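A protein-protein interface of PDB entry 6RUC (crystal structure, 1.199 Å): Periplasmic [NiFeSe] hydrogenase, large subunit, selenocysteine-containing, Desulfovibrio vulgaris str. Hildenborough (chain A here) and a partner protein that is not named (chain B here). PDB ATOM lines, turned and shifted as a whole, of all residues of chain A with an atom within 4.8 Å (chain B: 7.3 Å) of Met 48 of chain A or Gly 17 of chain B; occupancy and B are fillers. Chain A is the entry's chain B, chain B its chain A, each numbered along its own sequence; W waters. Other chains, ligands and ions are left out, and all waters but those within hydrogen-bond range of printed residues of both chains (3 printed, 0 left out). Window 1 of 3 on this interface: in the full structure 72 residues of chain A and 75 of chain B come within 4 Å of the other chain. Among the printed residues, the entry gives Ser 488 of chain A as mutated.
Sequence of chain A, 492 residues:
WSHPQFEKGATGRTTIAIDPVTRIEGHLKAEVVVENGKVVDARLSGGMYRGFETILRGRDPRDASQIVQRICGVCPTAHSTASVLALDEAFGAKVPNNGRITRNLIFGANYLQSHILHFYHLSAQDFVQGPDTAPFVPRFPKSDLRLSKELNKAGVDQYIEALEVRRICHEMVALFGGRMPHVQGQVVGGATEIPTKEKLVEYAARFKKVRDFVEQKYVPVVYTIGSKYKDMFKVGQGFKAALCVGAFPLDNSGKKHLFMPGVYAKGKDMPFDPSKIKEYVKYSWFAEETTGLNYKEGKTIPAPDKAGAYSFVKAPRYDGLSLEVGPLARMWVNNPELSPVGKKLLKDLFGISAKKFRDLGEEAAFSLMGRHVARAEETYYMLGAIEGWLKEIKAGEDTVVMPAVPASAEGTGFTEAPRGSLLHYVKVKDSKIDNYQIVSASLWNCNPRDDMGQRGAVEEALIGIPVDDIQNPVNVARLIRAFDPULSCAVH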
ATOM      1  N   HIS A  27     -13.529  -4.008  10.468  1.00  0.00           N
ATOM      2  CA  HIS A  27     -14.163  -2.685  10.481  1.00  0.00           C
ATOM      3  C   HIS A  27     -14.268  -2.175  11.915  1.00  0.00           C
ATOM      4  O   HIS A  27     -15.103  -2.656  12.694  1.00  0.00           O
ATOM      5  CB  HIS A  27     -15.558  -2.755   9.861  1.00  0.00           C
ATOM      6  CG  HIS A  27     -15.580  -3.270   8.461  1.00  0.00           C
ATOM      7  ND1 HIS A  27     -15.359  -4.595   8.140  1.00  0.00           N
ATOM      8  CD2 HIS A  27     -15.832  -2.635   7.295  1.00  0.00           C
ATOM      9  CE1 HIS A  27     -15.465  -4.749   6.834  1.00  0.00           C
ATOM     10  NE2 HIS A  27     -15.734  -3.574   6.294  1.00  0.00           N
ATOM     11  N   GLY A  46     -17.434  -2.067  16.426  1.00  0.00           N
ATOM     12  CA  GLY A  46     -17.296  -3.009  15.331  1.00  0.00           C
ATOM     13  C   GLY A  46     -18.408  -2.754  14.332  1.00  0.00           C
ATOM     14  O   GLY A  46     -19.591  -2.824  14.690  1.00  0.00           O
ATOM     15  N   GLY A  47     -18.052  -2.464  13.085  1.00  0.00           N
ATOM     16  CA  GLY A  47     -18.954  -1.834  12.149  1.00  0.00           C
ATOM     17  C   GLY A  47     -19.564  -2.694  11.067  1.00  0.00           C
ATOM     18  O   GLY A  47     -20.347  -2.165  10.270  1.00  0.00           O
ATOM     19  N   MET A  48     -19.263  -3.994  11.013  1.00  0.00           N
ATOM     20  CA  MET A  48     -19.766  -4.851   9.935  1.00  0.00           C
ATOM     21  C   MET A  48     -20.280  -6.169  10.497  1.00  0.00           C
ATOM     22  O   MET A  48     -19.581  -6.848  11.257  1.00  0.00           O
ATOM     23  CB  MET A  48     -18.681  -5.087   8.867  1.00  0.00           C
ATOM     24  CG  MET A  48     -19.131  -5.910   7.663  1.00  0.00           C
ATOM     25  SD  MET A  48     -19.100  -7.704   7.922  1.00  0.00           S
ATOM     26  CE  MET A  48     -17.340  -8.009   7.965  1.00  0.00           C
ATOM     27  N   TYR A  49     -21.512  -6.515  10.132  1.00  0.00           N
ATOM     28  CA  TYR A  49     -22.187  -7.702  10.636  1.00  0.00           C
ATOM     29  C   TYR A  49     -22.602  -8.593   9.478  1.00  0.00           C
ATOM     30  O   TYR A  49     -23.102  -8.105   8.456  1.00  0.00           O
ATOM     31  CB  TYR A  49     -23.434  -7.277  11.416  1.00  0.00           C
ATOM     32  CG  TYR A  49     -24.329  -8.404  11.895  1.00  0.00           C
ATOM     33  CD1 TYR A  49     -24.040  -9.103  13.061  1.00  0.00           C
ATOM     34  CD2 TYR A  49     -25.468  -8.770  11.182  1.00  0.00           C
ATOM     35  CE1 TYR A  49     -24.863 -10.132  13.514  1.00  0.00           C
ATOM     36  CE2 TYR A  49     -26.302  -9.804  11.626  1.00  0.00           C
ATOM     37  CZ  TYR A  49     -25.986 -10.484  12.788  1.00  0.00           C
ATOM     38  OH  TYR A  49     -26.799 -11.500  13.266  1.00  0.00           O
ATOM     39  N   ARG A  50     -22.420  -9.898   9.659  1.00  0.00           N
ATOM     40  CA  ARG A  50     -22.911 -10.911   8.726  1.00  0.00           C
ATOM     41  C   ARG A  50     -23.903 -11.897   9.337  1.00  0.00           C
ATOM     42  O   ARG A  50     -24.814 -12.338   8.638  1.00  0.00           O
ATOM     43  CB  ARG A  50     -21.725 -11.659   8.113  1.00  0.00           C
ATOM     44  CG  ARG A  50     -20.940 -10.771   7.147  1.00  0.00           C
ATOM     45  CD  ARG A  50     -19.537 -11.260   6.834  1.00  0.00           C
ATOM     46  NE  ARG A  50     -18.753 -11.311   8.057  1.00  0.00           N
ATOM     47  CZ  ARG A  50     -17.673 -12.058   8.245  1.00  0.00           C
ATOM     48  NH1 ARG A  50     -17.193 -12.791   7.253  1.00  0.00           N
ATOM     49  NH2 ARG A  50     -17.069 -12.087   9.438  1.00  0.00           N
ATOM     50  N   PHE A 312     -21.513  -3.808  16.800  1.00  0.00           N
ATOM     51  CA  PHE A 312     -22.032  -5.143  16.520  1.00  0.00           C
ATOM     52  C   PHE A 312     -21.313  -6.238  17.311  1.00  0.00           C
ATOM     53  O   PHE A 312     -21.648  -7.419  17.159  1.00  0.00           O
ATOM     54  CB  PHE A 312     -21.969  -5.449  15.014  1.00  0.00           C
ATOM     55  CG  PHE A 312     -22.997  -4.713  14.179  1.00  0.00           C
ATOM     56  CD1 PHE A 312     -24.354  -4.984  14.310  1.00  0.00           C
ATOM     57  CD2 PHE A 312     -22.604  -3.787  13.225  1.00  0.00           C
ATOM     58  CE1 PHE A 312     -25.306  -4.322  13.538  1.00  0.00           C
ATOM     59  CE2 PHE A 312     -23.539  -3.126  12.453  1.00  0.00           C
ATOM     60  CZ  PHE A 312     -24.902  -3.397  12.615  1.00  0.00           C
ATOM     61  N   SER A 488     -13.836  -8.819  12.140  1.00  0.00           N
ATOM     62  CA  SER A 488     -14.688  -9.819  11.506  1.00  0.00           C
ATOM     63  C   SER A 488     -14.879 -11.035  12.417  1.00  0.00           C
ATOM     64  O   SER A 488     -15.995 -11.557  12.542  1.00  0.00           O
ATOM     65  CB  SER A 488     -14.125 -10.191  10.133  1.00  0.00           C
ATOM     66  OG  SER A 488     -14.017  -9.025   9.313  1.00  0.00           O
ATOM     67  N   VAL A 491     -17.330  -9.853  15.455  1.00  0.00           N
ATOM     68  CA  VAL A 491     -18.756  -9.698  15.154  1.00  0.00           C
ATOM     69  C   VAL A 491     -19.363 -10.971  14.571  1.00  0.00           C
ATOM     70  O   VAL A 491     -20.481 -11.348  14.935  1.00  0.00           O
ATOM     71  CB  VAL A 491     -18.985  -8.505  14.199  1.00  0.00           C
ATOM     72  CG1 VAL A 491     -20.476  -8.399  13.857  1.00  0.00           C
ATOM     73  CG2 VAL A 491     -18.472  -7.203  14.808  1.00  0.00           C
ATOM     74  N   GLN B  14     -13.486  -3.069   1.573  1.00  0.00           N
ATOM     75  CA  GLN B  14     -14.010  -4.271   2.199  1.00  0.00           C
ATOM     76  C   GLN B  14     -15.434  -4.012   2.661  1.00  0.00           C
ATOM     77  O   GLN B  14     -15.677  -3.114   3.480  1.00  0.00           O
ATOM     78  CB  GLN B  14     -13.125  -4.700   3.367  1.00  0.00           C
ATOM     79  CG  GLN B  14     -11.742  -5.080   2.886  1.00  0.00           C
ATOM     80  CD  GLN B  14     -10.755  -5.386   3.983  1.00  0.00           C
ATOM     81  OE1 GLN B  14     -10.805  -4.820   5.071  1.00  0.00           O
ATOM     82  NE2 GLN B  14      -9.821  -6.272   3.688  1.00  0.00           N
ATOM     83  N   GLY B  15     -16.366  -4.771   2.101  1.00  0.00           N
ATOM     84  CA  GLY B  15     -17.728  -4.818   2.590  1.00  0.00           C
ATOM     85  C   GLY B  15     -17.871  -5.960   3.574  1.00  0.00           C
ATOM     86  O   GLY B  15     -17.106  -6.043   4.539  1.00  0.00           O
ATOM     87  N   GLN B  16     -18.837  -6.844   3.343  1.00  0.00           N
ATOM     88  CA  GLN B  16     -19.021  -8.034   4.176  1.00  0.00           C
ATOM     89  C   GLN B  16     -18.071  -9.143   3.734  1.00  0.00           C
ATOM     90  O   GLN B  16     -18.478 -10.177   3.202  1.00  0.00           O
ATOM     91  CB  GLN B  16     -20.463  -8.504   4.103  1.00  0.00           C
ATOM     92  CG  GLN B  16     -21.440  -7.548   4.752  1.00  0.00           C
ATOM     93  CD  GLN B  16     -22.864  -7.940   4.460  1.00  0.00           C
ATOM     94  OE1 GLN B  16     -23.266  -8.026   3.294  1.00  0.00           O
ATOM     95  NE2 GLN B  16     -23.638  -8.237   5.508  1.00  0.00           N
ATOM     96  N   GLY B  17     -16.778  -8.861   3.893  1.00  0.00           N
ATOM     97  CA  GLY B  17     -15.728  -9.807   3.610  1.00  0.00           C
ATOM     98  C   GLY B  17     -15.116 -10.338   4.899  1.00  0.00           C
ATOM     99  O   GLY B  17     -15.431  -9.876   6.006  1.00  0.00           O
ATOM    100  N   CYS B  18     -14.214 -11.309   4.736  1.00  0.00           N
ATOM    101  CA  CYS B  18     -13.520 -11.926   5.857  1.00  0.00           C
ATOM    102  C   CYS B  18     -12.024 -11.640   5.834  1.00  0.00           C
ATOM    103  O   CYS B  18     -11.293 -12.161   6.681  1.00  0.00           O
ATOM    104  CB  CYS B  18     -13.742 -13.449   5.863  1.00  0.00           C
ATOM    105  SG  CYS B  18     -12.749 -14.355   4.625  1.00  0.00           S
ATOM    106  N   THR B  19     -11.556 -10.852   4.870  1.00  0.00           N
ATOM    107  CA  THR B  19     -10.147 -10.508   4.648  1.00  0.00           C
ATOM    108  C   THR B  19      -9.387 -11.672   3.993  1.00  0.00           C
ATOM    109  O   THR B  19      -8.217 -11.521   3.639  1.00  0.00           O
ATOM    110  CB  THR B  19      -9.501  -9.898   5.910  1.00  0.00           C
ATOM    111  OG1 THR B  19     -10.313  -8.777   6.295  1.00  0.00           O
ATOM    112  CG2 THR B  19      -8.095  -9.388   5.663  1.00  0.00           C
ATOM    113  N   GLY B  20     -10.060 -12.792   3.721  1.00  0.00           N
ATOM    114  CA  GLY B  20      -9.410 -13.910   3.060  1.00  0.00           C
ATOM    115  C   GLY B  20      -9.045 -13.648   1.616  1.00  0.00           C
ATOM    116  O   GLY B  20      -8.102 -14.257   1.100  1.00  0.00           O
ATOM    117  N   CYS B  21      -9.785 -12.771   0.938  1.00  0.00           N
ATOM    118  CA  CYS B  21      -9.426 -12.404  -0.426  1.00  0.00           C
ATOM    119  C   CYS B  21      -8.170 -11.535  -0.438  1.00  0.00           C
ATOM    120  O   CYS B  21      -7.327 -11.643  -1.345  1.00  0.00           O
ATOM    121  CB  CYS B  21     -10.625 -11.749  -1.117  1.00  0.00           C
ATOM    122  SG  CYS B  21     -11.978 -12.925  -1.562  1.00  0.00           S
ATOM    123  N   GLU B  77     -14.056  -6.452  -1.895  1.00  0.00           N
ATOM    124  CA  GLU B  77     -13.967  -7.714  -1.169  1.00  0.00           C
ATOM    125  C   GLU B  77     -15.151  -7.756  -0.212  1.00  0.00           C
ATOM    126  O   GLU B  77     -15.313  -6.843   0.606  1.00  0.00           O
ATOM    127  CB  GLU B  77     -12.636  -7.771  -0.402  1.00  0.00           C
ATOM    128  CG  GLU B  77     -12.500  -8.886   0.639  1.00  0.00           C
ATOM    129  CD  GLU B  77     -11.091  -8.982   1.252  1.00  0.00           C
ATOM    130  OE1 GLU B  77     -10.353  -7.961   1.282  1.00  0.00           O
ATOM    131  OE2 GLU B  77     -10.737 -10.091   1.731  1.00  0.00           O
ATOM    132  N   GLY B  78     -15.981  -8.794  -0.316  1.00  0.00           N
ATOM    133  CA  GLY B  78     -17.192  -8.893   0.478  1.00  0.00           C
ATOM    134  C   GLY B  78     -18.424  -8.398  -0.272  1.00  0.00           C
ATOM    135  O   GLY B  78     -18.336  -7.671  -1.260  1.00  0.00           O
ATOM    136  N   SER B  79     -19.603  -8.788   0.233  1.00  0.00           N
ATOM    137  CA  SER B  79     -20.890  -8.358  -0.299  1.00  0.00           C
ATOM    138  C   SER B  79     -21.274  -6.975   0.240  1.00  0.00           C
ATOM    139  O   SER B  79     -20.638  -6.426   1.147  1.00  0.00           O
ATOM    140  CB  SER B  79     -21.960  -9.407   0.010  1.00  0.00           C
ATOM    141  OG  SER B  79     -22.026  -9.677   1.400  1.00  0.00           O
ATOM    142  N   PRO B  81     -24.327  -4.976   1.965  1.00  0.00           N
ATOM    143  CA  PRO B  81     -25.635  -5.181   2.602  1.00  0.00           C
ATOM    144  C   PRO B  81     -26.514  -3.949   2.512  1.00  0.00           C
ATOM    145  O   PRO B  81     -26.104  -2.854   2.924  1.00  0.00           O
ATOM    146  CB  PRO B  81     -25.261  -5.507   4.049  1.00  0.00           C
ATOM    147  CG  PRO B  81     -23.993  -4.717   4.297  1.00  0.00           C
ATOM    148  CD  PRO B  81     -23.268  -4.696   2.957  1.00  0.00           C
ATOM    149  N   LYS B  87     -26.664   0.016   7.291  1.00  0.00           N
ATOM    150  CA  LYS B  87     -25.990   0.075   8.584  1.00  0.00           C
ATOM    151  C   LYS B  87     -25.225  -1.190   8.941  1.00  0.00           C
ATOM    152  O   LYS B  87     -24.426  -1.155   9.886  1.00  0.00           O
ATOM    153  CB  LYS B  87     -27.017   0.352   9.680  1.00  0.00           C
ATOM    154  CG  LYS B  87     -27.485   1.782   9.760  1.00  0.00           C
ATOM    155  CD  LYS B  87     -28.436   1.983  10.953  1.00  0.00           C
ATOM    156  CE  LYS B  87     -28.951   3.384  11.015  1.00  0.00           C
ATOM    157  NZ  LYS B  87     -29.903   3.530  12.158  1.00  0.00           N
ATOM    158  N   TYR B  88     -25.424  -2.297   8.217  1.00  0.00           N
ATOM    159  CA  TYR B  88     -24.699  -3.523   8.528  1.00  0.00           C
ATOM    160  C   TYR B  88     -23.259  -3.512   8.015  1.00  0.00           C
ATOM    161  O   TYR B  88     -22.531  -4.481   8.260  1.00  0.00           O
ATOM    162  CB  TYR B  88     -25.454  -4.757   8.022  1.00  0.00           C
ATOM    163  CG  TYR B  88     -26.719  -5.077   8.792  1.00  0.00           C
ATOM    164  CD1 TYR B  88     -26.675  -5.380  10.151  1.00  0.00           C
ATOM    165  CD2 TYR B  88     -27.956  -5.089   8.157  1.00  0.00           C
ATOM    166  CE1 TYR B  88     -27.832  -5.687  10.846  1.00  0.00           C
ATOM    167  CE2 TYR B  88     -29.108  -5.391   8.838  1.00  0.00           C
ATOM    168  CZ  TYR B  88     -29.045  -5.691  10.193  1.00  0.00           C
ATOM    169  OH  TYR B  88     -30.188  -6.011  10.909  1.00  0.00           O
ATOM    170  N   CYS B  89     -22.817  -2.450   7.327  1.00  0.00           N
ATOM    171  CA  CYS B  89     -21.397  -2.324   6.974  1.00  0.00           C
ATOM    172  C   CYS B  89     -21.028  -0.846   6.890  1.00  0.00           C
ATOM    173  O   CYS B  89     -21.362  -0.176   5.904  1.00  0.00           O
ATOM    174  CB  CYS B  89     -21.079  -3.023   5.666  1.00  0.00           C
ATOM    175  SG  CYS B  89     -19.311  -2.966   5.313  1.00  0.00           S
ATOM    176  N   ILE B  90     -20.354  -0.345   7.928  1.00  0.00           N
ATOM    177  CA  ILE B  90     -19.820   1.013   7.951  1.00  0.00           C
ATOM    178  C   ILE B  90     -18.313   0.926   7.732  1.00  0.00           C
ATOM    179  O   ILE B  90     -17.614   0.208   8.461  1.00  0.00           O
ATOM    180  CB  ILE B  90     -20.139   1.727   9.281  1.00  0.00           C
ATOM    181  CG1 ILE B  90     -21.657   1.834   9.507  1.00  0.00           C
ATOM    182  CG2 ILE B  90     -19.498   3.115   9.323  1.00  0.00           C
ATOM    183  CD1 ILE B  90     -22.420   2.580   8.420  1.00  0.00           C
ATOM    184  N   ILE B  91     -17.813   1.650   6.727  1.00  0.00           N
ATOM    185  CA  ILE B  91     -16.414   1.548   6.301  1.00  0.00           C
ATOM    186  C   ILE B  91     -15.562   2.739   6.719  1.00  0.00           C
ATOM    187  O   ILE B  91     -14.333   2.697   6.535  1.00  0.00           O
ATOM    188  CB  ILE B  91     -16.253   1.277   4.783  1.00  0.00           C
ATOM    189  CG1 ILE B  91     -16.616   2.485   3.912  1.00  0.00           C
ATOM    190  CG2 ILE B  91     -17.050   0.048   4.349  1.00  0.00           C
ATOM    191  CD1 ILE B  91     -15.887   2.470   2.592  1.00  0.00           C
ATOM    192  N   CYS B 121     -18.174 -13.683  -2.380  1.00  0.00           N
ATOM    193  CA  CYS B 121     -19.085 -12.742  -1.718  1.00  0.00           C
ATOM    194  C   CYS B 121     -19.380 -11.538  -2.609  1.00  0.00           C
ATOM    195  O   CYS B 121     -20.546 -11.186  -2.844  1.00  0.00           O
ATOM    196  CB  CYS B 121     -18.495 -12.242  -0.395  1.00  0.00           C
ATOM    197  SG  CYS B 121     -18.219 -13.475   0.880  1.00  0.00           S
ATOM    198  N   ALA B 122     -18.325 -10.875  -3.076  1.00  0.00           N
ATOM    199  CA  ALA B 122     -18.494  -9.700  -3.921  1.00  0.00           C
ATOM    200  C   ALA B 122     -19.110 -10.069  -5.266  1.00  0.00           C
ATOM    201  O   ALA B 122     -19.958  -9.337  -5.795  1.00  0.00           O
ATOM    202  CB  ALA B 122     -17.141  -9.019  -4.136  1.00  0.00           C
ATOM    203  N   PRO B 128     -22.485 -14.477   3.076  1.00  0.00           N
ATOM    204  CA  PRO B 128     -23.345 -13.466   3.716  1.00  0.00           C
ATOM    205  C   PRO B 128     -24.745 -13.378   3.138  1.00  0.00           C
ATOM    206  O   PRO B 128     -25.641 -12.873   3.819  1.00  0.00           O
ATOM    207  CB  PRO B 128     -22.566 -12.162   3.507  1.00  0.00           C
ATOM    208  CG  PRO B 128     -21.138 -12.600   3.445  1.00  0.00           C
ATOM    209  CD  PRO B 128     -21.194 -13.893   2.648  1.00  0.00           C
HETATM  210  O   HOH W   1     -25.487 -11.354   6.113  1.00  0.00           O
HETATM  211  O   HOH W   2     -17.699 -12.772   4.405  1.00  0.00           O
HETATM  212  O   HOH W   3     -13.866  -7.639   6.718  1.00  0.00           O
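O of Gln 14 of chain B lies within hydrogen-bond range of NE2 of His 27 of chain A.
NE2 of His 27 of chain A sits close to O of Gly 15 of chain B, at 3.3 Å.
O of Tyr 49 of chain A lies within hydrogen-bond range of NE2 of Gln 16 of chain B.
O of Tyr 88 of chain B is in hydrogen-bond range of N of Tyr 49 of chain A, at 2.9 Å.
The side-chain sulfur (SG) of Cys 89 of chain B sits at hydrogen-bond distance from a ring nitrogen (NE2) of His 27 of chain A (3.8 Å).
The backbone carbonyl oxygen of Gly 47 of chain A sits at hydrogen-bond distance from the backbone NH of Ile 90 of chain B (3.0 Å).
The side-chain amide nitrogen of Gln 14 of chain B is in hydrogen-bond range of the side-chain carboxylate of Glu 77 of chain B, at 3.0 Å.
The backbone NH (N) of Gly 15 of chain B is in hydrogen-bond range of the backbone carbonyl oxygen (O) of Glu 77 of chain B, 2.8 Å away.
N of Gly 47 of chain A sits at hydrogen-bond distance from O of His 27 of chain A (3.0 Å).
The backbone carbonyl oxygen (O) of Gly 46 of chain A is in hydrogen-bond range of the backbone NH (N) of Phe 312 of chain A.
The side-chain sulfur (SD) of Met 48 of chain A sits close to the guanidinium group (NE) of Arg 50 of chain A, 3.6 Å away.
O of Ser 488 of chain A lies within hydrogen-bond range of NH2 of Arg 50 of chain A.
Among the printed residues, pairs that only touch across the chains: His 27 of chain A with Ile 90 of chain B, Gly 47 of chain A with Tyr 88 of chain B, Gly 47 of chain A with Cys 89 of chain B, Met 48 of chain A with Gly 15 of chain B, Met 48 of chain A with Gln 16 of chain B, Met 48 of chain A with Gly 17 of chain B, Met 48 of chain A with Tyr 88 of chain B, Met 48 of chain A with Cys 89 of chain B, Arg 50 of chain A with Gln 16 of chain B, Arg 50 of chain A with Gly 17 of chain B, Arg 50 of chain A with Cys 18 of chain B, Arg 50 of chain A with Pro 128 of chain B, Phe 312 of chain A with Lys 87 of chain B, Phe 312 of chain A with Tyr 88 of chain B and Ser 488 of chain A with Gly 17 of chain B.
Gly 47 of chain A touches three residues of chain B.
Met 48 of chain A touches just these residues of chain B: Gly 15, Gln 16, Gly 17, Tyr 88 and Cys 89.
Of the printed residues of chain B, Phe 312 of chain A touches Lys 87 (3.4 Å) and Tyr 88 (3.6 Å).
Printed residues of chain A within 4 Å of Gln 16 of chain B: Met 48 (3.8 Å), Tyr 49 (3.0 Å) and Arg 50 (3.8 Å).
Of chain A, only Met 48 (3.3 Å), Arg 50 (3.6 Å) and Ser 488 (3.7 Å) come within 4 Å of Gly 17 of chain B.
Of the printed residues of chain A, Cys 18 of chain B touches Arg 50 (3.8 Å).
Of the printed residues of chain A, Cys 89 of chain B touches His 27, Gly 47 and Met 48.
Printed residues of chain A within 4 Å of Ile 90 of chain B: His 27 and Gly 47.
The nearest residue of chain B that does not touch Met 48 of chain A is Ile 90 of chain B (4.9 Å).
The nearest printed residue of chain A that does not touch Gly 17 of chain B is His 27 of chain A (5.2 Å).
Of the 20 printed residues of chain B, 10 touch a printed residue of chain A.
Hydrophobic or aromatic side chains of chain B that line the printed part of chain A: Tyr 88 and Pro 128.
Printed residues of chain A that touch a printed residue of chain B: His 27, Gly 47, Met 48, Tyr 49, Arg 50, Phe 312 and Ser 488.
Hydrophobic or aromatic side chains of chain A that line the printed part of chain B: His 27, Met 48, Tyr 49 and Phe 312.
Among the printed residues, 21 pairs touch across the chains.
Among the printed residues, no Asp or Glu carboxylate lies within 4 Å of a Lys or Arg side-chain nitrogen of the other chain.
Water W1 bridges the backbone carbonyl oxygen of Pro 128 of chain B (2.8 Å) and the backbone carbonyl oxygen of Arg 50 of chain A (2.8 Å).
Water W3 bridges O of Gly 17 of chain B and OG of Ser 488 of chain A.
Water W2 lies within hydrogen-bond range of the guanidinium group of Arg 50 of chain A and the backbone carbonyl oxygen of Gln 16 of chain B.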
